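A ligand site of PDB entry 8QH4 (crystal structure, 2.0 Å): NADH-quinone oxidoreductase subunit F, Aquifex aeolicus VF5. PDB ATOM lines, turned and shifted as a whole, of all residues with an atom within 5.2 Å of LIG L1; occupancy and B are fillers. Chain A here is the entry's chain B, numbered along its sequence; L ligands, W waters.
OG1 of Thr 223 lies within hydrogen-bond range of O8 of LIG L1. O7 of LIG L1 lies within salt-bridge range of NZ of Lys 76. An oxygen (O9) of LIG L1 lies within hydrogen-bond range of the backbone NH of Gly 67 (2.7 Å). N of Asn 220 sits at hydrogen-bond distance from O8 of LIG L1 (2.9 Å). The side-chain amide nitrogen (ND2) of Asn 220 lies within hydrogen-bond range of an oxygen (O1) of LIG L1 (2.7 Å). ND2 of Asn 219 sits at hydrogen-bond distance from O8 of LIG L1 (3.0 Å). N of Glu 185 is in hydrogen-bond range of O3 of LIG L1 (3.1 Å). N of Glu 95 sits at hydrogen-bond distance from O2 of LIG L1 (3.1 Å). O5 of LIG L1 lies close to ND2 of Asn 92 (3.2 Å). N4 of LIG L1 lies close to O of Gly 183 (3.4 Å). An oxygen (O9) of LIG L1 is in hydrogen-bond range of the backbone NH (N) of Arg 66. O5 of LG2 L2 lies within hydrogen-bond range of NZ of Lys 76 (2.9 Å). OE2 of Glu 185 is in hydrogen-bond range of O6 of LG2 L2 (2.5 Å). The backbone carbonyl oxygen (O) of Gly 68 lies within hydrogen-bond range of an oxygen (O12) of LG2 L2, 3.1 Å away. The side-chain amino group (NZ) of Lys 202 lies within salt-bridge range of an oxygen (O8) of LG2 L2.
An oxygen (O8) of LG2 L2 sits at hydrogen-bond distance from an oxygen (O4) of LIG L1, 2.7 Å away.
The side-chain hydroxyl (OG1) of Thr 223 lies within hydrogen-bond range of the backbone NH (N) of Arg 66 (2.8 Å). The side-chain amino group (NZ) of Lys 76 lies within hydrogen-bond range of the backbone carbonyl oxygen (O) of Val 218, 2.7 Å away. The backbone carbonyl oxygen (O) of Asn 219 sits at hydrogen-bond distance from the backbone NH (N) of Asn 92 (2.8 Å). O of Asn 92 lies within hydrogen-bond range of N of Val 221, at 3.4 Å. OD2 of Asp 94 lies within hydrogen-bond range of N of Gly 183 (3.1 Å). The backbone carbonyl oxygen (O) of Phe 71 sits at hydrogen-bond distance from the backbone NH (N) of Gly 65. The backbone carbonyl oxygen (O) of Asp 94 sits at hydrogen-bond distance from the side-chain hydroxyl (OG) of Ser 96 (2.7 Å). N of Leu 395 lies close to SG of Cys 393, at 3.5 Å.
Water W5 lies within hydrogen-bond range of O9 of LIG L1 (2.6 Å), N of Ala 69 (3.0 Å) and N of Gly 68 (3.4 Å). Water W7 lies within hydrogen-bond range of an oxygen (O2) of LIG L1 (2.6 Å) and the backbone NH (N) of Ser 96 (3.1 Å). Water W6 lies within hydrogen-bond range of an oxygen (O7) of LIG L1 (2.7 Å), the backbone NH (N) of Phe 71 (2.9 Å) and the backbone NH (N) of Gly 70 (3.4 Å). Water W4 lies within hydrogen-bond range of O7 of LIG L1, O of Phe 71, ND2 of Asn 219 and N of Gly 65. Water W2 lies within hydrogen-bond range of OH of Tyr 180 (2.8 Å) and N4 of LIG L1 (3.4 Å).
An oxygen (O6) of LIG L1 lies close to the backbone carbonyl oxygen of Val 218 (3.5 Å). CA of Gly 65 touches O9 of LIG L1 (3.4 Å). Asp 94 touches LIG L1. N of Ser 96 touches O2 of LIG L1, at 3.9 Å. Tyr 180 touches LIG L1 (CE2 to C9, 3.6 Å). CD1 of Ile 181 touches C9 of LIG L1 (3.7 Å). N of Glu 184 touches C6 of LIG L1, 3.5 Å away. CA of Gly 394 touches C11 of LIG L1 (3.7 Å). Leu 395 touches LIG L1. Within 4 Å of LIG L1: Gly 65, Arg 66, Gly 67, Lys 76, Asn 92, Asp 94, Glu 95, Ser 96, Tyr 180, Ile 181, Gly 183, Glu 184, Glu 185, Val 218, Asn 219, Asn 220, Thr 223, Gly 394 and Leu 395. The nearest printed residue that does not touch LIG L1 is Gly 68 (4.2 Å).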
ATOM      1  N   GLY A  65      16.676  15.827  29.256  1.00  0.00           N
ATOM      2  CA  GLY A  65      16.768  14.464  29.729  1.00  0.00           C
ATOM      3  C   GLY A  65      18.004  13.740  29.177  1.00  0.00           C
ATOM      4  O   GLY A  65      18.299  13.849  27.982  1.00  0.00           O
ATOM      5  N   ARG A  66      18.695  13.019  30.054  1.00  0.00           N
ATOM      6  CA  ARG A  66      19.909  12.301  29.692  1.00  0.00           C
ATOM      7  C   ARG A  66      19.661  10.805  29.502  1.00  0.00           C
ATOM      8  O   ARG A  66      20.608  10.023  29.441  1.00  0.00           O
ATOM      9  CB  ARG A  66      20.943  12.491  30.815  1.00  0.00           C
ATOM     10  CG  ARG A  66      21.271  13.931  31.155  1.00  0.00           C
ATOM     11  CD  ARG A  66      22.048  14.640  30.062  1.00  0.00           C
ATOM     12  NE  ARG A  66      22.731  15.817  30.564  1.00  0.00           N
ATOM     13  CZ  ARG A  66      22.507  17.065  30.182  1.00  0.00           C
ATOM     14  NH1 ARG A  66      23.352  18.020  30.541  1.00  0.00           N
ATOM     15  NH2 ARG A  66      21.475  17.349  29.405  1.00  0.00           N
ATOM     16  N   GLY A  67      18.386  10.388  29.429  1.00  0.00           N
ATOM     17  CA  GLY A  67      18.069   8.971  29.297  1.00  0.00           C
ATOM     18  C   GLY A  67      17.959   8.528  27.837  1.00  0.00           C
ATOM     19  O   GLY A  67      17.713   7.351  27.559  1.00  0.00           O
ATOM     20  N   GLY A  68      18.076   9.495  26.907  1.00  0.00           N
ATOM     21  CA  GLY A  68      18.113   9.168  25.494  1.00  0.00           C
ATOM     22  C   GLY A  68      17.282  10.112  24.615  1.00  0.00           C
ATOM     23  O   GLY A  68      17.679  10.347  23.473  1.00  0.00           O
ATOM     24  N   ALA A  69      16.166  10.652  25.124  1.00  0.00           N
ATOM     25  CA  ALA A  69      15.215  11.392  24.295  1.00  0.00           C
ATOM     26  C   ALA A  69      15.425  12.904  24.376  1.00  0.00           C
ATOM     27  O   ALA A  69      14.920  13.628  23.516  1.00  0.00           O
ATOM     28  CB  ALA A  69      13.792  11.021  24.674  1.00  0.00           C
ATOM     29  N   GLY A  70      16.119  13.403  25.401  1.00  0.00           N
ATOM     30  CA  GLY A  70      16.450  14.823  25.480  1.00  0.00           C
ATOM     31  C   GLY A  70      15.254  15.746  25.729  1.00  0.00           C
ATOM     32  O   GLY A  70      15.311  16.928  25.367  1.00  0.00           O
ATOM     33  N   PHE A  71      14.205  15.271  26.404  1.00  0.00           N
ATOM     34  CA  PHE A  71      13.063  16.120  26.709  1.00  0.00           C
ATOM     35  C   PHE A  71      13.478  17.146  27.776  1.00  0.00           C
ATOM     36  O   PHE A  71      14.208  16.826  28.727  1.00  0.00           O
ATOM     37  CB  PHE A  71      11.839  15.283  27.098  1.00  0.00           C
ATOM     38  CG  PHE A  71      10.543  16.058  27.172  1.00  0.00           C
ATOM     39  CD1 PHE A  71      10.172  16.701  28.336  1.00  0.00           C
ATOM     40  CD2 PHE A  71       9.724  16.201  26.057  1.00  0.00           C
ATOM     41  CE1 PHE A  71       8.996  17.436  28.415  1.00  0.00           C
ATOM     42  CE2 PHE A  71       8.547  16.945  26.130  1.00  0.00           C
ATOM     43  CZ  PHE A  71       8.180  17.564  27.312  1.00  0.00           C
ATOM     44  N   LYS A  76       8.932  19.084  31.732  1.00  0.00           N
ATOM     45  CA  LYS A  76       8.320  17.831  32.165  1.00  0.00           C
ATOM     46  C   LYS A  76       7.703  18.022  33.545  1.00  0.00           C
ATOM     47  O   LYS A  76       6.571  17.614  33.788  1.00  0.00           O
ATOM     48  CB  LYS A  76       9.328  16.690  32.174  1.00  0.00           C
ATOM     49  CG  LYS A  76       8.699  15.310  32.322  1.00  0.00           C
ATOM     50  CD  LYS A  76       9.683  14.190  32.581  1.00  0.00           C
ATOM     51  CE  LYS A  76      10.670  13.973  31.453  1.00  0.00           C
ATOM     52  NZ  LYS A  76      11.431  12.714  31.647  1.00  0.00           N
ATOM     53  N   ASN A  92      15.112   6.598  37.067  1.00  0.00           N
ATOM     54  CA  ASN A  92      15.322   5.461  36.163  1.00  0.00           C
ATOM     55  C   ASN A  92      16.801   5.092  36.156  1.00  0.00           C
ATOM     56  O   ASN A  92      17.632   5.782  35.554  1.00  0.00           O
ATOM     57  CB  ASN A  92      14.812   5.782  34.760  1.00  0.00           C
ATOM     58  CG  ASN A  92      14.796   4.582  33.834  1.00  0.00           C
ATOM     59  OD1 ASN A  92      15.428   3.563  34.101  1.00  0.00           O
ATOM     60  ND2 ASN A  92      14.058   4.709  32.730  1.00  0.00           N
ATOM     61  N   ASP A  94      17.743   1.882  35.130  1.00  0.00           N
ATOM     62  CA  ASP A  94      17.679   0.576  34.485  1.00  0.00           C
ATOM     63  C   ASP A  94      18.863   0.341  33.535  1.00  0.00           C
ATOM     64  O   ASP A  94      19.141  -0.806  33.185  1.00  0.00           O
ATOM     65  CB  ASP A  94      16.360   0.343  33.750  1.00  0.00           C
ATOM     66  CG  ASP A  94      16.137  -1.132  33.479  1.00  0.00           C
ATOM     67  OD1 ASP A  94      16.091  -1.899  34.469  1.00  0.00           O
ATOM     68  OD2 ASP A  94      16.062  -1.516  32.291  1.00  0.00           O
ATOM     69  N   GLU A  95      19.529   1.420  33.123  1.00  0.00           N
ATOM     70  CA  GLU A  95      20.667   1.438  32.211  1.00  0.00           C
ATOM     71  C   GLU A  95      21.056   0.028  31.724  1.00  0.00           C
ATOM     72  O   GLU A  95      21.821  -0.675  32.381  1.00  0.00           O
ATOM     73  CB  GLU A  95      21.838   2.132  32.918  1.00  0.00           C
ATOM     74  CG  GLU A  95      23.110   2.164  32.103  1.00  0.00           C
ATOM     75  CD  GLU A  95      24.182   3.044  32.709  1.00  0.00           C
ATOM     76  OE1 GLU A  95      24.795   2.602  33.705  1.00  0.00           O
ATOM     77  OE2 GLU A  95      24.387   4.192  32.197  1.00  0.00           O
ATOM     78  N   SER A  96      20.550  -0.346  30.539  1.00  0.00           N
ATOM     79  CA  SER A  96      20.775  -1.667  29.984  1.00  0.00           C
ATOM     80  C   SER A  96      21.052  -1.639  28.482  1.00  0.00           C
ATOM     81  O   SER A  96      21.178  -2.686  27.868  1.00  0.00           O
ATOM     82  CB  SER A  96      19.586  -2.555  30.274  1.00  0.00           C
ATOM     83  OG  SER A  96      19.597  -2.976  31.626  1.00  0.00           O
ATOM     84  N   ASP A 103      25.578   5.824  34.052  1.00  0.00           N
ATOM     85  CA  ASP A 103      24.774   6.068  35.249  1.00  0.00           C
ATOM     86  C   ASP A 103      25.337   5.294  36.449  1.00  0.00           C
ATOM     87  O   ASP A 103      25.261   5.730  37.587  1.00  0.00           O
ATOM     88  CB  ASP A 103      23.312   5.657  35.032  1.00  0.00           C
ATOM     89  CG  ASP A 103      22.556   6.474  33.990  1.00  0.00           C
ATOM     90  OD1 ASP A 103      23.046   7.539  33.613  1.00  0.00           O
ATOM     91  OD2 ASP A 103      21.464   6.027  33.568  1.00  0.00           O
ATOM     92  N   TYR A 180      15.413  -5.358  29.470  1.00  0.00           N
ATOM     93  CA  TYR A 180      15.815  -4.045  28.976  1.00  0.00           C
ATOM     94  C   TYR A 180      14.629  -3.098  28.832  1.00  0.00           C
ATOM     95  O   TYR A 180      14.762  -1.883  29.031  1.00  0.00           O
ATOM     96  CB  TYR A 180      16.525  -4.181  27.620  1.00  0.00           C
ATOM     97  CG  TYR A 180      16.653  -2.909  26.826  1.00  0.00           C
ATOM     98  CD1 TYR A 180      17.464  -1.872  27.256  1.00  0.00           C
ATOM     99  CD2 TYR A 180      15.995  -2.744  25.619  1.00  0.00           C
ATOM    100  CE1 TYR A 180      17.594  -0.700  26.531  1.00  0.00           C
ATOM    101  CE2 TYR A 180      16.104  -1.578  24.888  1.00  0.00           C
ATOM    102  CZ  TYR A 180      16.915  -0.542  25.335  1.00  0.00           C
ATOM    103  OH  TYR A 180      17.046   0.622  24.616  1.00  0.00           O
ATOM    104  N   ILE A 181      13.461  -3.661  28.491  1.00  0.00           N
ATOM    105  CA  ILE A 181      12.276  -2.873  28.224  1.00  0.00           C
ATOM    106  C   ILE A 181      11.797  -2.173  29.494  1.00  0.00           C
ATOM    107  O   ILE A 181      11.000  -1.250  29.405  1.00  0.00           O
ATOM    108  CB  ILE A 181      11.145  -3.736  27.601  1.00  0.00           C
ATOM    109  CG1 ILE A 181      10.042  -2.878  26.977  1.00  0.00           C
ATOM    110  CG2 ILE A 181      10.575  -4.722  28.620  1.00  0.00           C
ATOM    111  CD1 ILE A 181      10.517  -1.966  25.871  1.00  0.00           C
ATOM    112  N   GLY A 183      13.440  -0.215  31.224  1.00  0.00           N
ATOM    113  CA  GLY A 183      13.928   1.151  31.175  1.00  0.00           C
ATOM    114  C   GLY A 183      12.955   2.096  30.452  1.00  0.00           C
ATOM    115  O   GLY A 183      13.031   3.311  30.628  1.00  0.00           O
ATOM    116  N   GLU A 184      12.083   1.551  29.595  1.00  0.00           N
ATOM    117  CA  GLU A 184      11.036   2.364  28.999  1.00  0.00           C
ATOM    118  C   GLU A 184      10.100   2.767  30.135  1.00  0.00           C
ATOM    119  O   GLU A 184       9.701   1.920  30.929  1.00  0.00           O
ATOM    120  CB  GLU A 184      10.306   1.584  27.896  1.00  0.00           C
ATOM    121  CG  GLU A 184       9.466   2.440  26.981  1.00  0.00           C
ATOM    122  CD  GLU A 184       8.078   2.845  27.479  1.00  0.00           C
ATOM    123  OE1 GLU A 184       7.631   2.319  28.496  1.00  0.00           O
ATOM    124  OE2 GLU A 184       7.467   3.707  26.822  1.00  0.00           O
ATOM    125  N   GLU A 185       9.766   4.045  30.227  1.00  0.00           N
ATOM    126  CA  GLU A 185       9.260   4.588  31.489  1.00  0.00           C
ATOM    127  C   GLU A 185       7.920   3.949  31.870  1.00  0.00           C
ATOM    128  O   GLU A 185       7.649   3.777  33.058  1.00  0.00           O
ATOM    129  CB  GLU A 185       9.146   6.108  31.405  1.00  0.00           C
ATOM    130  CG  GLU A 185       8.328   6.579  30.214  1.00  0.00           C
ATOM    131  CD  GLU A 185       8.144   8.088  30.112  1.00  0.00           C
ATOM    132  OE1 GLU A 185       8.751   8.829  30.938  1.00  0.00           O
ATOM    133  OE2 GLU A 185       7.392   8.507  29.220  1.00  0.00           O
ATOM    134  N   LYS A 202       1.169   5.612  24.939  1.00  0.00           N
ATOM    135  CA  LYS A 202       1.366   7.020  25.261  1.00  0.00           C
ATOM    136  C   LYS A 202       0.892   7.873  24.084  1.00  0.00           C
ATOM    137  O   LYS A 202       1.176   7.522  22.935  1.00  0.00           O
ATOM    138  CB  LYS A 202       2.856   7.343  25.505  1.00  0.00           C
ATOM    139  CG  LYS A 202       3.523   6.644  26.683  1.00  0.00           C
ATOM    140  CD  LYS A 202       4.878   7.246  27.076  1.00  0.00           C
ATOM    141  CE  LYS A 202       6.009   6.979  26.091  1.00  0.00           C
ATOM    142  NZ  LYS A 202       7.349   7.304  26.654  1.00  0.00           N
ATOM    143  N   VAL A 218       9.263  10.571  35.553  1.00  0.00           N
ATOM    144  CA  VAL A 218      10.403   9.691  35.432  1.00  0.00           C
ATOM    145  C   VAL A 218      11.569  10.484  34.870  1.00  0.00           C
ATOM    146  O   VAL A 218      11.422  11.152  33.851  1.00  0.00           O
ATOM    147  CB  VAL A 218      10.111   8.470  34.535  1.00  0.00           C
ATOM    148  CG1 VAL A 218      11.321   7.554  34.471  1.00  0.00           C
ATOM    149  CG2 VAL A 218       8.868   7.708  35.000  1.00  0.00           C
ATOM    150  N   ASN A 219      12.729  10.393  35.527  1.00  0.00           N
ATOM    151  CA  ASN A 219      13.940  11.031  35.049  1.00  0.00           C
ATOM    152  C   ASN A 219      15.109  10.061  35.198  1.00  0.00           C
ATOM    153  O   ASN A 219      15.157   9.234  36.118  1.00  0.00           O
ATOM    154  CB  ASN A 219      14.260  12.350  35.762  1.00  0.00           C
ATOM    155  CG  ASN A 219      13.555  13.552  35.174  1.00  0.00           C
ATOM    156  OD1 ASN A 219      12.884  14.280  35.908  1.00  0.00           O
ATOM    157  ND2 ASN A 219      13.708  13.794  33.883  1.00  0.00           N
ATOM    158  N   ASN A 220      16.065  10.195  34.283  1.00  0.00           N
ATOM    159  CA  ASN A 220      17.274   9.378  34.255  1.00  0.00           C
ATOM    160  C   ASN A 220      18.208   9.805  35.387  1.00  0.00           C
ATOM    161  O   ASN A 220      18.170  10.970  35.800  1.00  0.00           O
ATOM    162  CB  ASN A 220      17.923   9.501  32.879  1.00  0.00           C
ATOM    163  CG  ASN A 220      19.291   8.865  32.794  1.00  0.00           C
ATOM    164  OD1 ASN A 220      20.293   9.572  32.850  1.00  0.00           O
ATOM    165  ND2 ASN A 220      19.318   7.541  32.738  1.00  0.00           N
ATOM    166  N   VAL A 221      19.030   8.860  35.879  1.00  0.00           N
ATOM    167  CA  VAL A 221      20.052   9.079  36.904  1.00  0.00           C
ATOM    168  C   VAL A 221      20.847  10.349  36.615  1.00  0.00           C
ATOM    169  O   VAL A 221      20.950  11.212  37.497  1.00  0.00           O
ATOM    170  CB  VAL A 221      20.993   7.864  37.017  1.00  0.00           C
ATOM    171  CG1 VAL A 221      22.251   8.166  37.829  1.00  0.00           C
ATOM    172  CG2 VAL A 221      20.278   6.635  37.578  1.00  0.00           C
ATOM    173  N   THR A 223      20.326  12.871  34.513  1.00  0.00           N
ATOM    174  CA  THR A 223      19.485  14.052  34.595  1.00  0.00           C
ATOM    175  C   THR A 223      19.394  14.544  36.045  1.00  0.00           C
ATOM    176  O   THR A 223      19.663  15.712  36.341  1.00  0.00           O
ATOM    177  CB  THR A 223      18.072  13.777  34.051  1.00  0.00           C
ATOM    178  OG1 THR A 223      18.143  13.086  32.794  1.00  0.00           O
ATOM    179  CG2 THR A 223      17.261  15.041  33.909  1.00  0.00           C
ATOM    180  N   CYS A 393       5.839   1.429  21.664  1.00  0.00           N
ATOM    181  CA  CYS A 393       6.978   2.053  22.347  1.00  0.00           C
ATOM    182  C   CYS A 393       8.162   2.190  21.402  1.00  0.00           C
ATOM    183  O   CYS A 393       8.108   1.767  20.242  1.00  0.00           O
ATOM    184  CB  CYS A 393       7.374   1.345  23.641  1.00  0.00           C
ATOM    185  SG  CYS A 393       8.610   0.017  23.474  1.00  0.00           S
ATOM    186  N   GLY A 394       9.204   2.839  21.912  1.00  0.00           N
ATOM    187  CA  GLY A 394      10.355   3.252  21.126  1.00  0.00           C
ATOM    188  C   GLY A 394      11.226   2.102  20.622  1.00  0.00           C
ATOM    189  O   GLY A 394      11.969   2.275  19.651  1.00  0.00           O
ATOM    190  N   LEU A 395      11.139   0.936  21.278  1.00  0.00           N
ATOM    191  CA  LEU A 395      11.954  -0.216  20.890  1.00  0.00           C
ATOM    192  C   LEU A 395      11.602  -0.671  19.466  1.00  0.00           C
ATOM    193  O   LEU A 395      12.491  -0.845  18.634  1.00  0.00           O
ATOM    194  CB  LEU A 395      11.774  -1.334  21.917  1.00  0.00           C
ATOM    195  CG  LEU A 395      12.736  -2.509  21.765  1.00  0.00           C
ATOM    196  CD1 LEU A 395      12.962  -3.219  23.094  1.00  0.00           C
ATOM    197  CD2 LEU A 395      12.209  -3.499  20.722  1.00  0.00           C
HETATM  198  C1  LIG L   1      14.207   3.929  27.466  1.00  0.00           C
HETATM  199  N1  LIG L   1      14.568   5.025  28.309  1.00  0.00           N
HETATM  200  C2  LIG L   1      15.504   4.813  29.317  1.00  0.00           C
HETATM  201  N2  LIG L   1      15.769   5.832  30.195  1.00  0.00           N
HETATM  202  C3  LIG L   1      16.641   5.714  31.245  1.00  0.00           C
HETATM  203  O1  LIG L   1      16.827   6.636  32.035  1.00  0.00           O
HETATM  204  N3  LIG L   1      17.239   4.489  31.383  1.00  0.00           N
HETATM  205  C4  LIG L   1      17.061   3.375  30.579  1.00  0.00           C
HETATM  206  O2  LIG L   1      17.715   2.355  30.806  1.00  0.00           O
HETATM  207  C5  LIG L   1      16.104   3.580  29.513  1.00  0.00           C
HETATM  208  N4  LIG L   1      15.757   2.539  28.711  1.00  0.00           N
HETATM  209  C6  LIG L   1      14.789   2.679  27.713  1.00  0.00           C
HETATM  210  C7  LIG L   1      14.436   1.580  26.933  1.00  0.00           C
HETATM  211  C8  LIG L   1      13.506   1.706  25.906  1.00  0.00           C
HETATM  212  C9  LIG L   1      13.195   0.514  25.039  1.00  0.00           C
HETATM  213  C10 LIG L   1      12.923   2.963  25.653  1.00  0.00           C
HETATM  214  C11 LIG L   1      11.968   3.153  24.494  1.00  0.00           C
HETATM  215  C12 LIG L   1      13.262   4.061  26.433  1.00  0.00           C
HETATM  216  C13 LIG L   1      13.921   6.329  28.172  1.00  0.00           C
HETATM  217  C14 LIG L   1      12.761   6.456  29.173  1.00  0.00           C
HETATM  218  O3  LIG L   1      11.586   5.891  28.583  1.00  0.00           O
HETATM  219  C15 LIG L   1      12.512   7.934  29.498  1.00  0.00           C
HETATM  220  O4  LIG L   1      12.575   8.726  28.312  1.00  0.00           O
HETATM  221  C16 LIG L   1      13.522   8.568  30.471  1.00  0.00           C
HETATM  222  O5  LIG L   1      13.772   7.736  31.603  1.00  0.00           O
HETATM  223  C17 LIG L   1      13.054   9.932  30.929  1.00  0.00           C
HETATM  224  O6  LIG L   1      14.110  10.535  31.704  1.00  0.00           O
HETATM  225  P1  LIG L   1      14.964  11.793  31.103  1.00  0.00           P
HETATM  226  O7  LIG L   1      13.941  12.786  30.601  1.00  0.00           O
HETATM  227  O8  LIG L   1      15.728  12.301  32.318  1.00  0.00           O
HETATM  228  O9  LIG L   1      15.864  11.245  30.012  1.00  0.00           O
HETATM  229  P1  LG2 L   2       9.836  10.172  24.337  1.00  0.00           P
HETATM  230  O1  LG2 L   2      10.316  11.193  23.372  1.00  0.00           O
HETATM  231  O2  LG2 L   2       8.524   9.520  24.111  1.00  0.00           O
HETATM  232  O3  LG2 L   2       9.756  10.880  25.778  1.00  0.00           O
HETATM  233  C1  LG2 L   2      10.906  11.423  26.466  1.00  0.00           C
HETATM  234  C2  LG2 L   2      10.462  11.888  27.831  1.00  0.00           C
HETATM  235  O4  LG2 L   2       9.674  13.089  27.682  1.00  0.00           O
HETATM  236  C3  LG2 L   2       9.582  10.912  28.615  1.00  0.00           C
HETATM  237  O5  LG2 L   2       9.753  11.089  30.013  1.00  0.00           O
HETATM  238  C4  LG2 L   2       8.165  11.336  28.212  1.00  0.00           C
HETATM  239  O6  LG2 L   2       7.171  11.026  29.200  1.00  0.00           O
HETATM  240  C5  LG2 L   2       8.345  12.855  28.114  1.00  0.00           C
HETATM  241  N1  LG2 L   2       7.440  13.479  27.162  1.00  0.00           N
HETATM  242  C6  LG2 L   2       7.519  13.447  25.793  1.00  0.00           C
HETATM  243  N2  LG2 L   2       6.549  14.086  25.176  1.00  0.00           N
HETATM  244  C7  LG2 L   2       5.777  14.584  26.220  1.00  0.00           C
HETATM  245  C8  LG2 L   2       4.603  15.357  26.247  1.00  0.00           C
HETATM  246  N3  LG2 L   2       3.938  15.759  25.153  1.00  0.00           N
HETATM  247  N4  LG2 L   2       4.087  15.677  27.455  1.00  0.00           N
HETATM  248  C9  LG2 L   2       4.719  15.257  28.566  1.00  0.00           C
HETATM  249  N5  LG2 L   2       5.830  14.523  28.661  1.00  0.00           N
HETATM  250  C10 LG2 L   2       6.314  14.223  27.454  1.00  0.00           C
HETATM  251  O7  LG2 L   2      10.983   9.058  24.462  1.00  0.00           O
HETATM  252  P2  LG2 L   2      11.070   7.581  25.073  1.00  0.00           P
HETATM  253  O8  LG2 L   2      10.858   7.650  26.541  1.00  0.00           O
HETATM  254  O9  LG2 L   2      10.249   6.651  24.252  1.00  0.00           O
HETATM  255  O10 LG2 L   2      12.611   7.266  24.882  1.00  0.00           O
HETATM  256  C11 LG2 L   2      13.157   6.981  23.576  1.00  0.00           C
HETATM  257  C12 LG2 L   2      14.664   6.949  23.678  1.00  0.00           C
HETATM  258  O11 LG2 L   2      15.101   5.714  24.296  1.00  0.00           O
HETATM  259  C13 LG2 L   2      15.375   7.040  22.330  1.00  0.00           C
HETATM  260  O12 LG2 L   2      15.721   8.396  22.068  1.00  0.00           O
HETATM  261  C14 LG2 L   2      16.603   6.152  22.549  1.00  0.00           C
HETATM  262  O13 LG2 L   2      17.671   6.866  23.165  1.00  0.00           O
HETATM  263  C15 LG2 L   2      16.004   5.064  23.446  1.00  0.00           C
HETATM  264  N6  LG2 L   2      15.266   4.010  22.657  1.00  0.00           N
HETATM  265  O   HOH W   1      16.909  -0.299  30.079  1.00  0.00           O
HETATM  266  O   HOH W   2      17.910   2.905  26.048  1.00  0.00           O
HETATM  267  O   HOH W   3      19.220   4.447  33.607  1.00  0.00           O
HETATM  268  O   HOH W   4      13.866  15.447  31.160  1.00  0.00           O
HETATM  269  O   HOH W   5      14.870  10.291  27.800  1.00  0.00           O
HETATM  270  O   HOH W   6      13.857  12.854  27.929  1.00  0.00           O
HETATM  271  O   HOH W   7      19.347   1.916  28.777  1.00  0.00           O
